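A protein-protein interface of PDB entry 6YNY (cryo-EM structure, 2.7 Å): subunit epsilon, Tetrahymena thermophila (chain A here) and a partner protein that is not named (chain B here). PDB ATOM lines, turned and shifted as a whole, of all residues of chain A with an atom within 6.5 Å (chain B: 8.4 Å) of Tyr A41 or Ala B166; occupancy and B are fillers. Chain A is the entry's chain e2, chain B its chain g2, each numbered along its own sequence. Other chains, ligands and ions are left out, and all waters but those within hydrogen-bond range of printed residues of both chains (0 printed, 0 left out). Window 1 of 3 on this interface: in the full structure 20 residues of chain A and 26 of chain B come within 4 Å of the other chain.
O of Val B154 sits at hydrogen-bond distance from N of Thr A42, at 2.8 Å. OE1 of Gln B157 sits close to O of Asn A40 (2.7 Å). The side-chain amide oxygen (OE1) of Gln B157 lies within hydrogen-bond range of the backbone NH (N) of Tyr A41.
The backbone carbonyl oxygen of Asn B155 sits at hydrogen-bond distance from the side-chain amide nitrogen of Gln B157, at 2.6 Å. O of Tyr A41 lies within hydrogen-bond range of N of Lys A55. O of Val A43 lies within hydrogen-bond range of N of Ser A53, 2.6 Å away.
Among the printed residues, pairs that only touch across the chains: Val A15 with Ala B165 (3.8 Å), Val A15 with Glu B233 (3.7 Å), Ile A39 with Pro B162 (3.1 Å), Ile A39 with Thr B163 (3.2 Å), Asn A40 with Asn B155 (3.7 Å), Asn A40 with Ile B156 (3.9 Å), Tyr A41 with Ile B153 (3.5 Å), Tyr A41 with Val B154 (3.9 Å), Tyr A41 with Asn B155 (3.4 Å), Tyr A41 with Ala B166 (3.8 Å), Tyr A41 with Ile B167 (3.6 Å), Thr A42 with Ser B152 (3.9 Å), Thr A42 with Ile B153 (3.3 Å), Thr A42 with Asn B155 (3.3 Å), Val A43 with Ser B152 (3.3 Å), Ala A63 with Ala B166 (3.8 Å), Ala A63 with His B169 (3.8 Å), Phe A64 with Pro B162 (3.8 Å), Phe A64 with Ala B165 (3.2 Å), Phe A64 with Ala B166 (3.2 Å) and Phe A64 with His B169 (3.6 Å).
Of chain B, only Ile B153 (3.5 Å), Val B154 (3.9 Å), Asn B155 (3.4 Å), Gln B157 (3.5 Å), Ala B166 (3.8 Å) and Ile B167 (3.6 Å) come within 4 Å of Tyr A41. Ala B166 touches three residues of chain A. Of the printed residues of chain A, Asn B155 touches Asn A40, Tyr A41 and Thr A42. Printed residues of chain A within 4 Å of Pro B162: Ile A39 (3.1 Å) and Phe A64 (3.8 Å). Printed residues of chain A within 4 Å of Ile B156: Asn A40. Of the printed residues of chain A, Ile B167 touches Tyr A41. Thr A56 touches none of the printed residues of chain B. Ala B164 touches none of the printed residues of chain A. The nearest printed residue of chain B that does not touch Tyr A41 is Ile B156 (4.2 Å). The nearest residue of chain A that does not touch Ala B166 is Ile A39 (4.4 Å). The nearest printed residue of chain A that does not touch Pro B162 is Val A15 (4.8 Å).
Hydrophobic or aromatic side chains of chain B within 4 Å of the printed part of chain A: Ile B153, Pro B162, Ala B165, Ala B166, Ile B167 and His B169. Among the printed residues, 24 pairs touch across the chains.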
ATOM      1  N   VAL A  15     -22.958 -15.364  32.345  1.00  0.00           N
ATOM      2  CA  VAL A  15     -23.973 -15.777  31.379  1.00  0.00           C
ATOM      3  C   VAL A  15     -24.598 -17.097  31.805  1.00  0.00           C
ATOM      4  O   VAL A  15     -25.826 -17.246  31.824  1.00  0.00           O
ATOM      5  CB  VAL A  15     -23.363 -15.870  29.970  1.00  0.00           C
ATOM      6  CG1 VAL A  15     -24.399 -16.361  28.977  1.00  0.00           C
ATOM      7  CG2 VAL A  15     -22.810 -14.522  29.544  1.00  0.00           C
ATOM      8  N   ILE A  39     -29.329 -22.912  22.784  1.00  0.00           N
ATOM      9  CA  ILE A  39     -27.967 -23.049  22.285  1.00  0.00           C
ATOM     10  C   ILE A  39     -27.811 -24.456  21.730  1.00  0.00           C
ATOM     11  O   ILE A  39     -27.947 -25.437  22.472  1.00  0.00           O
ATOM     12  CB  ILE A  39     -26.918 -22.780  23.377  1.00  0.00           C
ATOM     13  CG1 ILE A  39     -27.081 -21.361  23.928  1.00  0.00           C
ATOM     14  CG2 ILE A  39     -25.513 -22.981  22.820  1.00  0.00           C
ATOM     15  CD1 ILE A  39     -26.168 -21.044  25.093  1.00  0.00           C
ATOM     16  N   ASN A  40     -27.520 -24.556  20.435  1.00  0.00           N
ATOM     17  CA  ASN A  40     -27.348 -25.852  19.780  1.00  0.00           C
ATOM     18  C   ASN A  40     -26.362 -25.669  18.637  1.00  0.00           C
ATOM     19  O   ASN A  40     -26.699 -25.059  17.618  1.00  0.00           O
ATOM     20  CB  ASN A  40     -28.679 -26.399  19.272  1.00  0.00           C
ATOM     21  CG  ASN A  40     -29.599 -26.835  20.393  1.00  0.00           C
ATOM     22  OD1 ASN A  40     -29.157 -27.410  21.387  1.00  0.00           O
ATOM     23  ND2 ASN A  40     -30.890 -26.569  20.235  1.00  0.00           N
ATOM     24  N   TYR A  41     -25.151 -26.191  18.806  1.00  0.00           N
ATOM     25  CA  TYR A  41     -24.137 -26.136  17.764  1.00  0.00           C
ATOM     26  C   TYR A  41     -23.283 -27.395  17.870  1.00  0.00           C
ATOM     27  O   TYR A  41     -23.583 -28.305  18.649  1.00  0.00           O
ATOM     28  CB  TYR A  41     -23.309 -24.851  17.881  1.00  0.00           C
ATOM     29  CG  TYR A  41     -22.535 -24.725  19.172  1.00  0.00           C
ATOM     30  CD1 TYR A  41     -21.165 -24.949  19.206  1.00  0.00           C
ATOM     31  CD2 TYR A  41     -23.172 -24.383  20.356  1.00  0.00           C
ATOM     32  CE1 TYR A  41     -20.452 -24.834  20.383  1.00  0.00           C
ATOM     33  CE2 TYR A  41     -22.467 -24.266  21.539  1.00  0.00           C
ATOM     34  CZ  TYR A  41     -21.108 -24.494  21.546  1.00  0.00           C
ATOM     35  OH  TYR A  41     -20.403 -24.381  22.721  1.00  0.00           O
ATOM     36  N   THR A  42     -22.213 -27.448  17.082  1.00  0.00           N
ATOM     37  CA  THR A  42     -21.370 -28.630  17.003  1.00  0.00           C
ATOM     38  C   THR A  42     -19.907 -28.217  17.014  1.00  0.00           C
ATOM     39  O   THR A  42     -19.527 -27.229  16.379  1.00  0.00           O
ATOM     40  CB  THR A  42     -21.672 -29.444  15.739  1.00  0.00           C
ATOM     41  OG1 THR A  42     -23.080 -29.701  15.660  1.00  0.00           O
ATOM     42  CG2 THR A  42     -20.923 -30.769  15.756  1.00  0.00           C
ATOM     43  N   VAL A  43     -19.094 -28.978  17.743  1.00  0.00           N
ATOM     44  CA  VAL A  43     -17.663 -28.731  17.864  1.00  0.00           C
ATOM     45  C   VAL A  43     -16.929 -29.991  17.434  1.00  0.00           C
ATOM     46  O   VAL A  43     -17.185 -31.078  17.966  1.00  0.00           O
ATOM     47  CB  VAL A  43     -17.269 -28.336  19.298  1.00  0.00           C
ATOM     48  CG1 VAL A  43     -15.781 -28.030  19.368  1.00  0.00           C
ATOM     49  CG2 VAL A  43     -18.090 -27.143  19.764  1.00  0.00           C
ATOM     50  N   SER A  53     -18.459 -33.252  18.384  1.00  0.00           N
ATOM     51  CA  SER A  53     -19.137 -32.982  19.645  1.00  0.00           C
ATOM     52  C   SER A  53     -20.342 -32.082  19.414  1.00  0.00           C
ATOM     53  O   SER A  53     -20.250 -31.081  18.697  1.00  0.00           O
ATOM     54  CB  SER A  53     -18.181 -32.327  20.642  1.00  0.00           C
ATOM     55  OG  SER A  53     -18.832 -32.056  21.868  1.00  0.00           O
ATOM     56  N   ALA A  54     -21.464 -32.439  20.031  1.00  0.00           N
ATOM     57  CA  ALA A  54     -22.707 -31.684  19.933  1.00  0.00           C
ATOM     58  C   ALA A  54     -22.936 -30.980  21.261  1.00  0.00           C
ATOM     59  O   ALA A  54     -23.053 -31.638  22.301  1.00  0.00           O
ATOM     60  CB  ALA A  54     -23.884 -32.596  19.592  1.00  0.00           C
ATOM     61  N   LYS A  55     -23.000 -29.653  21.228  1.00  0.00           N
ATOM     62  CA  LYS A  55     -23.170 -28.845  22.433  1.00  0.00           C
ATOM     63  C   LYS A  55     -24.631 -28.415  22.504  1.00  0.00           C
ATOM     64  O   LYS A  55     -25.068 -27.527  21.768  1.00  0.00           O
ATOM     65  CB  LYS A  55     -22.226 -27.647  22.417  1.00  0.00           C
ATOM     66  CG  LYS A  55     -20.858 -27.942  21.810  1.00  0.00           C
ATOM     67  CD  LYS A  55     -20.148 -29.103  22.499  1.00  0.00           C
ATOM     68  CE  LYS A  55     -19.739 -28.750  23.919  1.00  0.00           C
ATOM     69  NZ  LYS A  55     -18.979 -29.848  24.580  1.00  0.00           N
ATOM     70  N   THR A  56     -25.384 -29.055  23.397  1.00  0.00           N
ATOM     71  CA  THR A  56     -26.812 -28.805  23.538  1.00  0.00           C
ATOM     72  C   THR A  56     -27.271 -28.612  24.974  1.00  0.00           C
ATOM     73  O   THR A  56     -28.346 -28.035  25.179  1.00  0.00           O
ATOM     74  CB  THR A  56     -27.620 -29.956  22.921  1.00  0.00           C
ATOM     75  OG1 THR A  56     -27.324 -31.177  23.612  1.00  0.00           O
ATOM     76  CG2 THR A  56     -27.282 -30.115  21.446  1.00  0.00           C
ATOM     77  N   GLU A  62     -20.922 -28.086  29.547  1.00  0.00           N
ATOM     78  CA  GLU A  62     -21.062 -28.365  28.122  1.00  0.00           C
ATOM     79  C   GLU A  62     -20.713 -27.141  27.289  1.00  0.00           C
ATOM     80  O   GLU A  62     -19.837 -27.221  26.421  1.00  0.00           O
ATOM     81  CB  GLU A  62     -22.490 -28.837  27.822  1.00  0.00           C
ATOM     82  CG  GLU A  62     -22.691 -29.366  26.409  1.00  0.00           C
ATOM     83  CD  GLU A  62     -21.966 -30.674  26.164  1.00  0.00           C
ATOM     84  OE1 GLU A  62     -21.478 -31.279  27.142  1.00  0.00           O
ATOM     85  OE2 GLU A  62     -21.881 -31.098  24.991  1.00  0.00           O
ATOM     86  N   ALA A  63     -21.366 -26.005  27.532  1.00  0.00           N
ATOM     87  CA  ALA A  63     -21.080 -24.765  26.821  1.00  0.00           C
ATOM     88  C   ALA A  63     -20.203 -23.821  27.628  1.00  0.00           C
ATOM     89  O   ALA A  63     -19.261 -23.237  27.083  1.00  0.00           O
ATOM     90  CB  ALA A  63     -22.385 -24.054  26.456  1.00  0.00           C
ATOM     91  N   PHE A  64     -20.497 -23.656  28.919  1.00  0.00           N
ATOM     92  CA  PHE A  64     -19.726 -22.803  29.822  1.00  0.00           C
ATOM     93  C   PHE A  64     -19.154 -23.685  30.924  1.00  0.00           C
ATOM     94  O   PHE A  64     -19.758 -23.818  32.001  1.00  0.00           O
ATOM     95  CB  PHE A  64     -20.590 -21.685  30.402  1.00  0.00           C
ATOM     96  CG  PHE A  64     -21.166 -20.766  29.367  1.00  0.00           C
ATOM     97  CD1 PHE A  64     -20.377 -19.806  28.759  1.00  0.00           C
ATOM     98  CD2 PHE A  64     -22.499 -20.854  29.010  1.00  0.00           C
ATOM     99  CE1 PHE A  64     -20.905 -18.957  27.809  1.00  0.00           C
ATOM    100  CE2 PHE A  64     -23.033 -20.007  28.060  1.00  0.00           C
ATOM    101  CZ  PHE A  64     -22.235 -19.057  27.460  1.00  0.00           C
ATOM    102  N   VAL B 133     -14.482 -21.319  11.977  1.00  0.00           N
ATOM    103  CA  VAL B 133     -15.910 -21.368  12.263  1.00  0.00           C
ATOM    104  C   VAL B 133     -16.645 -21.532  10.939  1.00  0.00           C
ATOM    105  O   VAL B 133     -16.466 -20.720  10.025  1.00  0.00           O
ATOM    106  CB  VAL B 133     -16.402 -20.107  12.994  1.00  0.00           C
ATOM    107  CG1 VAL B 133     -17.869 -20.243  13.358  1.00  0.00           C
ATOM    108  CG2 VAL B 133     -15.560 -19.852  14.229  1.00  0.00           C
ATOM    109  N   SER B 152     -13.023 -26.598  15.631  1.00  0.00           N
ATOM    110  CA  SER B 152     -13.859 -25.630  14.939  1.00  0.00           C
ATOM    111  C   SER B 152     -15.294 -25.788  15.415  1.00  0.00           C
ATOM    112  O   SER B 152     -15.656 -26.784  16.048  1.00  0.00           O
ATOM    113  CB  SER B 152     -13.777 -25.803  13.420  1.00  0.00           C
ATOM    114  OG  SER B 152     -14.347 -27.037  13.019  1.00  0.00           O
ATOM    115  N   ILE B 153     -16.114 -24.788  15.100  1.00  0.00           N
ATOM    116  CA  ILE B 153     -17.530 -24.779  15.444  1.00  0.00           C
ATOM    117  C   ILE B 153     -18.326 -24.739  14.150  1.00  0.00           C
ATOM    118  O   ILE B 153     -18.050 -23.915  13.270  1.00  0.00           O
ATOM    119  CB  ILE B 153     -17.898 -23.586  16.345  1.00  0.00           C
ATOM    120  CG1 ILE B 153     -17.190 -23.690  17.699  1.00  0.00           C
ATOM    121  CG2 ILE B 153     -19.406 -23.526  16.534  1.00  0.00           C
ATOM    122  CD1 ILE B 153     -15.734 -23.265  17.677  1.00  0.00           C
ATOM    123  N   VAL B 154     -19.314 -25.625  14.038  1.00  0.00           N
ATOM    124  CA  VAL B 154     -20.142 -25.748  12.844  1.00  0.00           C
ATOM    125  C   VAL B 154     -21.536 -26.200  13.263  1.00  0.00           C
ATOM    126  O   VAL B 154     -21.789 -26.520  14.426  1.00  0.00           O
ATOM    127  CB  VAL B 154     -19.544 -26.737  11.820  1.00  0.00           C
ATOM    128  CG1 VAL B 154     -18.180 -26.259  11.356  1.00  0.00           C
ATOM    129  CG2 VAL B 154     -19.449 -28.132  12.420  1.00  0.00           C
ATOM    130  N   ASN B 155     -22.450 -26.221  12.294  1.00  0.00           N
ATOM    131  CA  ASN B 155     -23.812 -26.707  12.504  1.00  0.00           C
ATOM    132  C   ASN B 155     -24.528 -25.887  13.576  1.00  0.00           C
ATOM    133  O   ASN B 155     -25.094 -26.422  14.531  1.00  0.00           O
ATOM    134  CB  ASN B 155     -23.804 -28.192  12.867  1.00  0.00           C
ATOM    135  CG  ASN B 155     -23.177 -29.052  11.787  1.00  0.00           C
ATOM    136  OD1 ASN B 155     -23.249 -28.729  10.601  1.00  0.00           O
ATOM    137  ND2 ASN B 155     -22.554 -30.152  12.193  1.00  0.00           N
ATOM    138  N   ILE B 156     -24.496 -24.570  13.406  1.00  0.00           N
ATOM    139  CA  ILE B 156     -25.180 -23.658  14.315  1.00  0.00           C
ATOM    140  C   ILE B 156     -26.667 -23.675  13.984  1.00  0.00           C
ATOM    141  O   ILE B 156     -27.070 -23.329  12.869  1.00  0.00           O
ATOM    142  CB  ILE B 156     -24.605 -22.239  14.211  1.00  0.00           C
ATOM    143  CG1 ILE B 156     -23.112 -22.253  14.543  1.00  0.00           C
ATOM    144  CG2 ILE B 156     -25.356 -21.294  15.139  1.00  0.00           C
ATOM    145  CD1 ILE B 156     -22.433 -20.917  14.378  1.00  0.00           C
ATOM    146  N   GLN B 157     -27.487 -24.076  14.957  1.00  0.00           N
ATOM    147  CA  GLN B 157     -28.925 -24.143  14.720  1.00  0.00           C
ATOM    148  C   GLN B 157     -29.517 -22.750  14.544  1.00  0.00           C
ATOM    149  O   GLN B 157     -30.325 -22.523  13.635  1.00  0.00           O
ATOM    150  CB  GLN B 157     -29.610 -24.879  15.871  1.00  0.00           C
ATOM    151  CG  GLN B 157     -29.561 -26.397  15.757  1.00  0.00           C
ATOM    152  CD  GLN B 157     -28.153 -26.931  15.566  1.00  0.00           C
ATOM    153  OE1 GLN B 157     -27.498 -27.343  16.524  1.00  0.00           O
ATOM    154  NE2 GLN B 157     -27.681 -26.929  14.325  1.00  0.00           N
ATOM    155  N   ASN B 158     -29.132 -21.809  15.400  1.00  0.00           N
ATOM    156  CA  ASN B 158     -29.648 -20.450  15.323  1.00  0.00           C
ATOM    157  C   ASN B 158     -28.642 -19.511  15.966  1.00  0.00           C
ATOM    158  O   ASN B 158     -27.766 -19.936  16.724  1.00  0.00           O
ATOM    159  CB  ASN B 158     -31.014 -20.331  16.006  1.00  0.00           C
ATOM    160  CG  ASN B 158     -31.007 -20.878  17.421  1.00  0.00           C
ATOM    161  OD1 ASN B 158     -29.953 -21.017  18.041  1.00  0.00           O
ATOM    162  ND2 ASN B 158     -32.187 -21.194  17.938  1.00  0.00           N
ATOM    163  N   ASN B 160     -27.986 -16.477  18.487  1.00  0.00           N
ATOM    164  CA  ASN B 160     -28.548 -15.796  19.644  1.00  0.00           C
ATOM    165  C   ASN B 160     -27.425 -15.512  20.629  1.00  0.00           C
ATOM    166  O   ASN B 160     -26.368 -16.147  20.593  1.00  0.00           O
ATOM    167  CB  ASN B 160     -29.659 -16.623  20.298  1.00  0.00           C
ATOM    168  CG  ASN B 160     -29.186 -17.989  20.744  1.00  0.00           C
ATOM    169  OD1 ASN B 160     -28.326 -18.598  20.110  1.00  0.00           O
ATOM    170  ND2 ASN B 160     -29.750 -18.480  21.840  1.00  0.00           N
ATOM    171  N   PHE B 161     -27.669 -14.547  21.512  1.00  0.00           N
ATOM    172  CA  PHE B 161     -26.621 -14.117  22.431  1.00  0.00           C
ATOM    173  C   PHE B 161     -26.158 -15.240  23.349  1.00  0.00           C
ATOM    174  O   PHE B 161     -24.939 -15.371  23.551  1.00  0.00           O
ATOM    175  CB  PHE B 161     -27.101 -12.914  23.248  1.00  0.00           C
ATOM    176  CG  PHE B 161     -26.006 -12.229  24.007  1.00  0.00           C
ATOM    177  CD1 PHE B 161     -25.178 -11.314  23.380  1.00  0.00           C
ATOM    178  CD2 PHE B 161     -25.799 -12.502  25.346  1.00  0.00           C
ATOM    179  CE1 PHE B 161     -24.168 -10.683  24.073  1.00  0.00           C
ATOM    180  CE2 PHE B 161     -24.790 -11.874  26.046  1.00  0.00           C
ATOM    181  CZ  PHE B 161     -23.972 -10.964  25.407  1.00  0.00           C
ATOM    182  N   PRO B 162     -27.038 -16.063  23.925  1.00  0.00           N
ATOM    183  CA  PRO B 162     -26.551 -17.194  24.730  1.00  0.00           C
ATOM    184  C   PRO B 162     -25.576 -18.079  23.976  1.00  0.00           C
ATOM    185  O   PRO B 162     -24.553 -18.491  24.536  1.00  0.00           O
ATOM    186  CB  PRO B 162     -27.841 -17.942  25.091  1.00  0.00           C
ATOM    187  CG  PRO B 162     -28.906 -16.913  25.026  1.00  0.00           C
ATOM    188  CD  PRO B 162     -28.508 -15.982  23.925  1.00  0.00           C
ATOM    189  N   THR B 163     -25.865 -18.380  22.710  1.00  0.00           N
ATOM    190  CA  THR B 163     -24.942 -19.179  21.914  1.00  0.00           C
ATOM    191  C   THR B 163     -23.657 -18.409  21.639  1.00  0.00           C
ATOM    192  O   THR B 163     -22.555 -18.936  21.822  1.00  0.00           O
ATOM    193  CB  THR B 163     -25.608 -19.598  20.603  1.00  0.00           C
ATOM    194  OG1 THR B 163     -26.823 -20.302  20.884  1.00  0.00           O
ATOM    195  CG2 THR B 163     -24.682 -20.493  19.796  1.00  0.00           C
ATOM    196  N   ALA B 164     -23.781 -17.153  21.202  1.00  0.00           N
ATOM    197  CA  ALA B 164     -22.594 -16.348  20.936  1.00  0.00           C
ATOM    198  C   ALA B 164     -21.700 -16.257  22.164  1.00  0.00           C
ATOM    199  O   ALA B 164     -20.476 -16.148  22.035  1.00  0.00           O
ATOM    200  CB  ALA B 164     -22.998 -14.950  20.471  1.00  0.00           C
ATOM    201  N   ALA B 165     -22.289 -16.304  23.361  1.00  0.00           N
ATOM    202  CA  ALA B 165     -21.484 -16.305  24.577  1.00  0.00           C
ATOM    203  C   ALA B 165     -20.749 -17.628  24.739  1.00  0.00           C
ATOM    204  O   ALA B 165     -19.585 -17.652  25.157  1.00  0.00           O
ATOM    205  CB  ALA B 165     -22.367 -16.029  25.791  1.00  0.00           C
ATOM    206  N   ALA B 166     -21.411 -18.739  24.413  1.00  0.00           N
ATOM    207  CA  ALA B 166     -20.744 -20.035  24.469  1.00  0.00           C
ATOM    208  C   ALA B 166     -19.554 -20.069  23.522  1.00  0.00           C
ATOM    209  O   ALA B 166     -18.494 -20.606  23.861  1.00  0.00           O
ATOM    210  CB  ALA B 166     -21.732 -21.149  24.130  1.00  0.00           C
ATOM    211  N   ILE B 167     -19.711 -19.494  22.330  1.00  0.00           N
ATOM    212  CA  ILE B 167     -18.595 -19.408  21.397  1.00  0.00           C
ATOM    213  C   ILE B 167     -17.539 -18.451  21.931  1.00  0.00           C
ATOM    214  O   ILE B 167     -16.338 -18.740  21.885  1.00  0.00           O
ATOM    215  CB  ILE B 167     -19.096 -18.978  20.007  1.00  0.00           C
ATOM    216  CG1 ILE B 167     -20.257 -19.869  19.553  1.00  0.00           C
ATOM    217  CG2 ILE B 167     -17.963 -19.023  18.999  1.00  0.00           C
ATOM    218  CD1 ILE B 167     -19.990 -21.354  19.673  1.00  0.00           C
ATOM    219  N   ALA B 168     -17.967 -17.297  22.448  1.00  0.00           N
ATOM    220  CA  ALA B 168     -17.019 -16.354  23.029  1.00  0.00           C
ATOM    221  C   ALA B 168     -16.281 -16.981  24.202  1.00  0.00           C
ATOM    222  O   ALA B 168     -15.092 -16.716  24.415  1.00  0.00           O
ATOM    223  CB  ALA B 168     -17.746 -15.084  23.469  1.00  0.00           C
ATOM    224  N   HIS B 169     -16.973 -17.818  24.976  1.00  0.00           N
ATOM    225  CA  HIS B 169     -16.329 -18.486  26.100  1.00  0.00           C
ATOM    226  C   HIS B 169     -15.283 -19.482  25.616  1.00  0.00           C
ATOM    227  O   HIS B 169     -14.181 -19.552  26.169  1.00  0.00           O
ATOM    228  CB  HIS B 169     -17.379 -19.185  26.959  1.00  0.00           C
ATOM    229  CG  HIS B 169     -16.831 -19.787  28.212  1.00  0.00           C
ATOM    230  ND1 HIS B 169     -16.591 -19.049  29.351  1.00  0.00           N
ATOM    231  CD2 HIS B 169     -16.471 -21.058  28.506  1.00  0.00           C
ATOM    232  CE1 HIS B 169     -16.109 -19.839  30.293  1.00  0.00           C
ATOM    233  NE2 HIS B 169     -16.026 -21.064  29.806  1.00  0.00           N
ATOM    234  N   GLN B 170     -15.613 -20.261  24.584  1.00  0.00           N
ATOM    235  CA  GLN B 170     -14.648 -21.200  24.025  1.00  0.00           C
ATOM    236  C   GLN B 170     -13.413 -20.470  23.517  1.00  0.00           C
ATOM    237  O   GLN B 170     -12.277 -20.866  23.809  1.00  0.00           O
ATOM    238  CB  GLN B 170     -15.295 -22.010  22.905  1.00  0.00           C
ATOM    239  CG  GLN B 170     -15.729 -23.402  23.324  1.00  0.00           C
ATOM    240  CD  GLN B 170     -14.553 -24.309  23.630  1.00  0.00           C
ATOM    241  OE1 GLN B 170     -13.401 -23.956  23.380  1.00  0.00           O
ATOM    242  NE2 GLN B 170     -14.839 -25.486  24.174  1.00  0.00           N
ATOM    243  N   VAL B 171     -13.614 -19.400  22.746  1.00  0.00           N
ATOM    244  CA  VAL B 171     -12.484 -18.616  22.259  1.00  0.00           C
ATOM    245  C   VAL B 171     -11.662 -18.093  23.428  1.00  0.00           C
ATOM    246  O   VAL B 171     -10.433 -17.992  23.348  1.00  0.00           O
ATOM    247  CB  VAL B 171     -12.977 -17.469  21.362  1.00  0.00           C
ATOM    248  CG1 VAL B 171     -11.817 -16.573  20.961  1.00  0.00           C
ATOM    249  CG2 VAL B 171     -13.678 -18.021  20.135  1.00  0.00           C
ATOM    250  N   SER B 172     -12.328 -17.754  24.533  1.00  0.00           N
ATOM    251  CA  SER B 172     -11.608 -17.269  25.705  1.00  0.00           C
ATOM    252  C   SER B 172     -10.681 -18.344  26.254  1.00  0.00           C
ATOM    253  O   SER B 172      -9.536 -18.059  26.626  1.00  0.00           O
ATOM    254  CB  SER B 172     -12.596 -16.813  26.775  1.00  0.00           C
ATOM    255  OG  SER B 172     -11.918 -16.289  27.903  1.00  0.00           O
ATOM    256  N   THR B 173     -11.159 -19.589  26.315  1.00  0.00           N
ATOM    257  CA  THR B 173     -10.316 -20.678  26.797  1.00  0.00           C
ATOM    258  C   THR B 173      -9.120 -20.890  25.879  1.00  0.00           C
ATOM    259  O   THR B 173      -8.004 -21.144  26.349  1.00  0.00           O
ATOM    260  CB  THR B 173     -11.133 -21.966  26.909  1.00  0.00           C
ATOM    261  OG1 THR B 173     -11.635 -22.332  25.618  1.00  0.00           O
ATOM    262  CG2 THR B 173     -12.303 -21.781  27.869  1.00  0.00           C
ATOM    263  N   GLU B 233     -16.574 -11.008  29.534  1.00  0.00           N
ATOM    264  CA  GLU B 233     -17.505 -11.767  28.706  1.00  0.00           C
ATOM    265  C   GLU B 233     -18.309 -10.837  27.808  1.00  0.00           C
ATOM    266  O   GLU B 233     -18.402 -11.049  26.594  1.00  0.00           O
ATOM    267  CB  GLU B 233     -18.437 -12.590  29.593  1.00  0.00           C
ATOM    268  CG  GLU B 233     -17.733 -13.635  30.432  1.00  0.00           C
ATOM    269  CD  GLU B 233     -18.673 -14.334  31.394  1.00  0.00           C
ATOM    270  OE1 GLU B 233     -18.668 -13.983  32.593  1.00  0.00           O
ATOM    271  OE2 GLU B 233     -19.423 -15.226  30.949  1.00  0.00           O
ATOM    272  N   ALA B 237     -18.289 -11.442  24.031  1.00  0.00           N
ATOM    273  CA  ALA B 237     -19.520 -11.925  23.415  1.00  0.00           C
ATOM    274  C   ALA B 237     -20.135 -10.871  22.505  1.00  0.00           C
ATOM    275  O   ALA B 237     -20.719 -11.204  21.467  1.00  0.00           O
ATOM    276  CB  ALA B 237     -20.514 -12.346  24.495  1.00  0.00           C
ATOM    277  N   VAL B 240     -18.451 -11.138  19.128  1.00  0.00           N
ATOM    278  CA  VAL B 240     -18.820 -12.395  18.484  1.00  0.00           C
ATOM    279  C   VAL B 240     -20.269 -12.348  18.014  1.00  0.00           C
ATOM    280  O   VAL B 240     -20.577 -12.676  16.862  1.00  0.00           O
ATOM    281  CB  VAL B 240     -18.582 -13.574  19.444  1.00  0.00           C
ATOM    282  CG1 VAL B 240     -19.165 -14.851  18.874  1.00  0.00           C
ATOM    283  CG2 VAL B 240     -17.100 -13.738  19.716  1.00  0.00           C
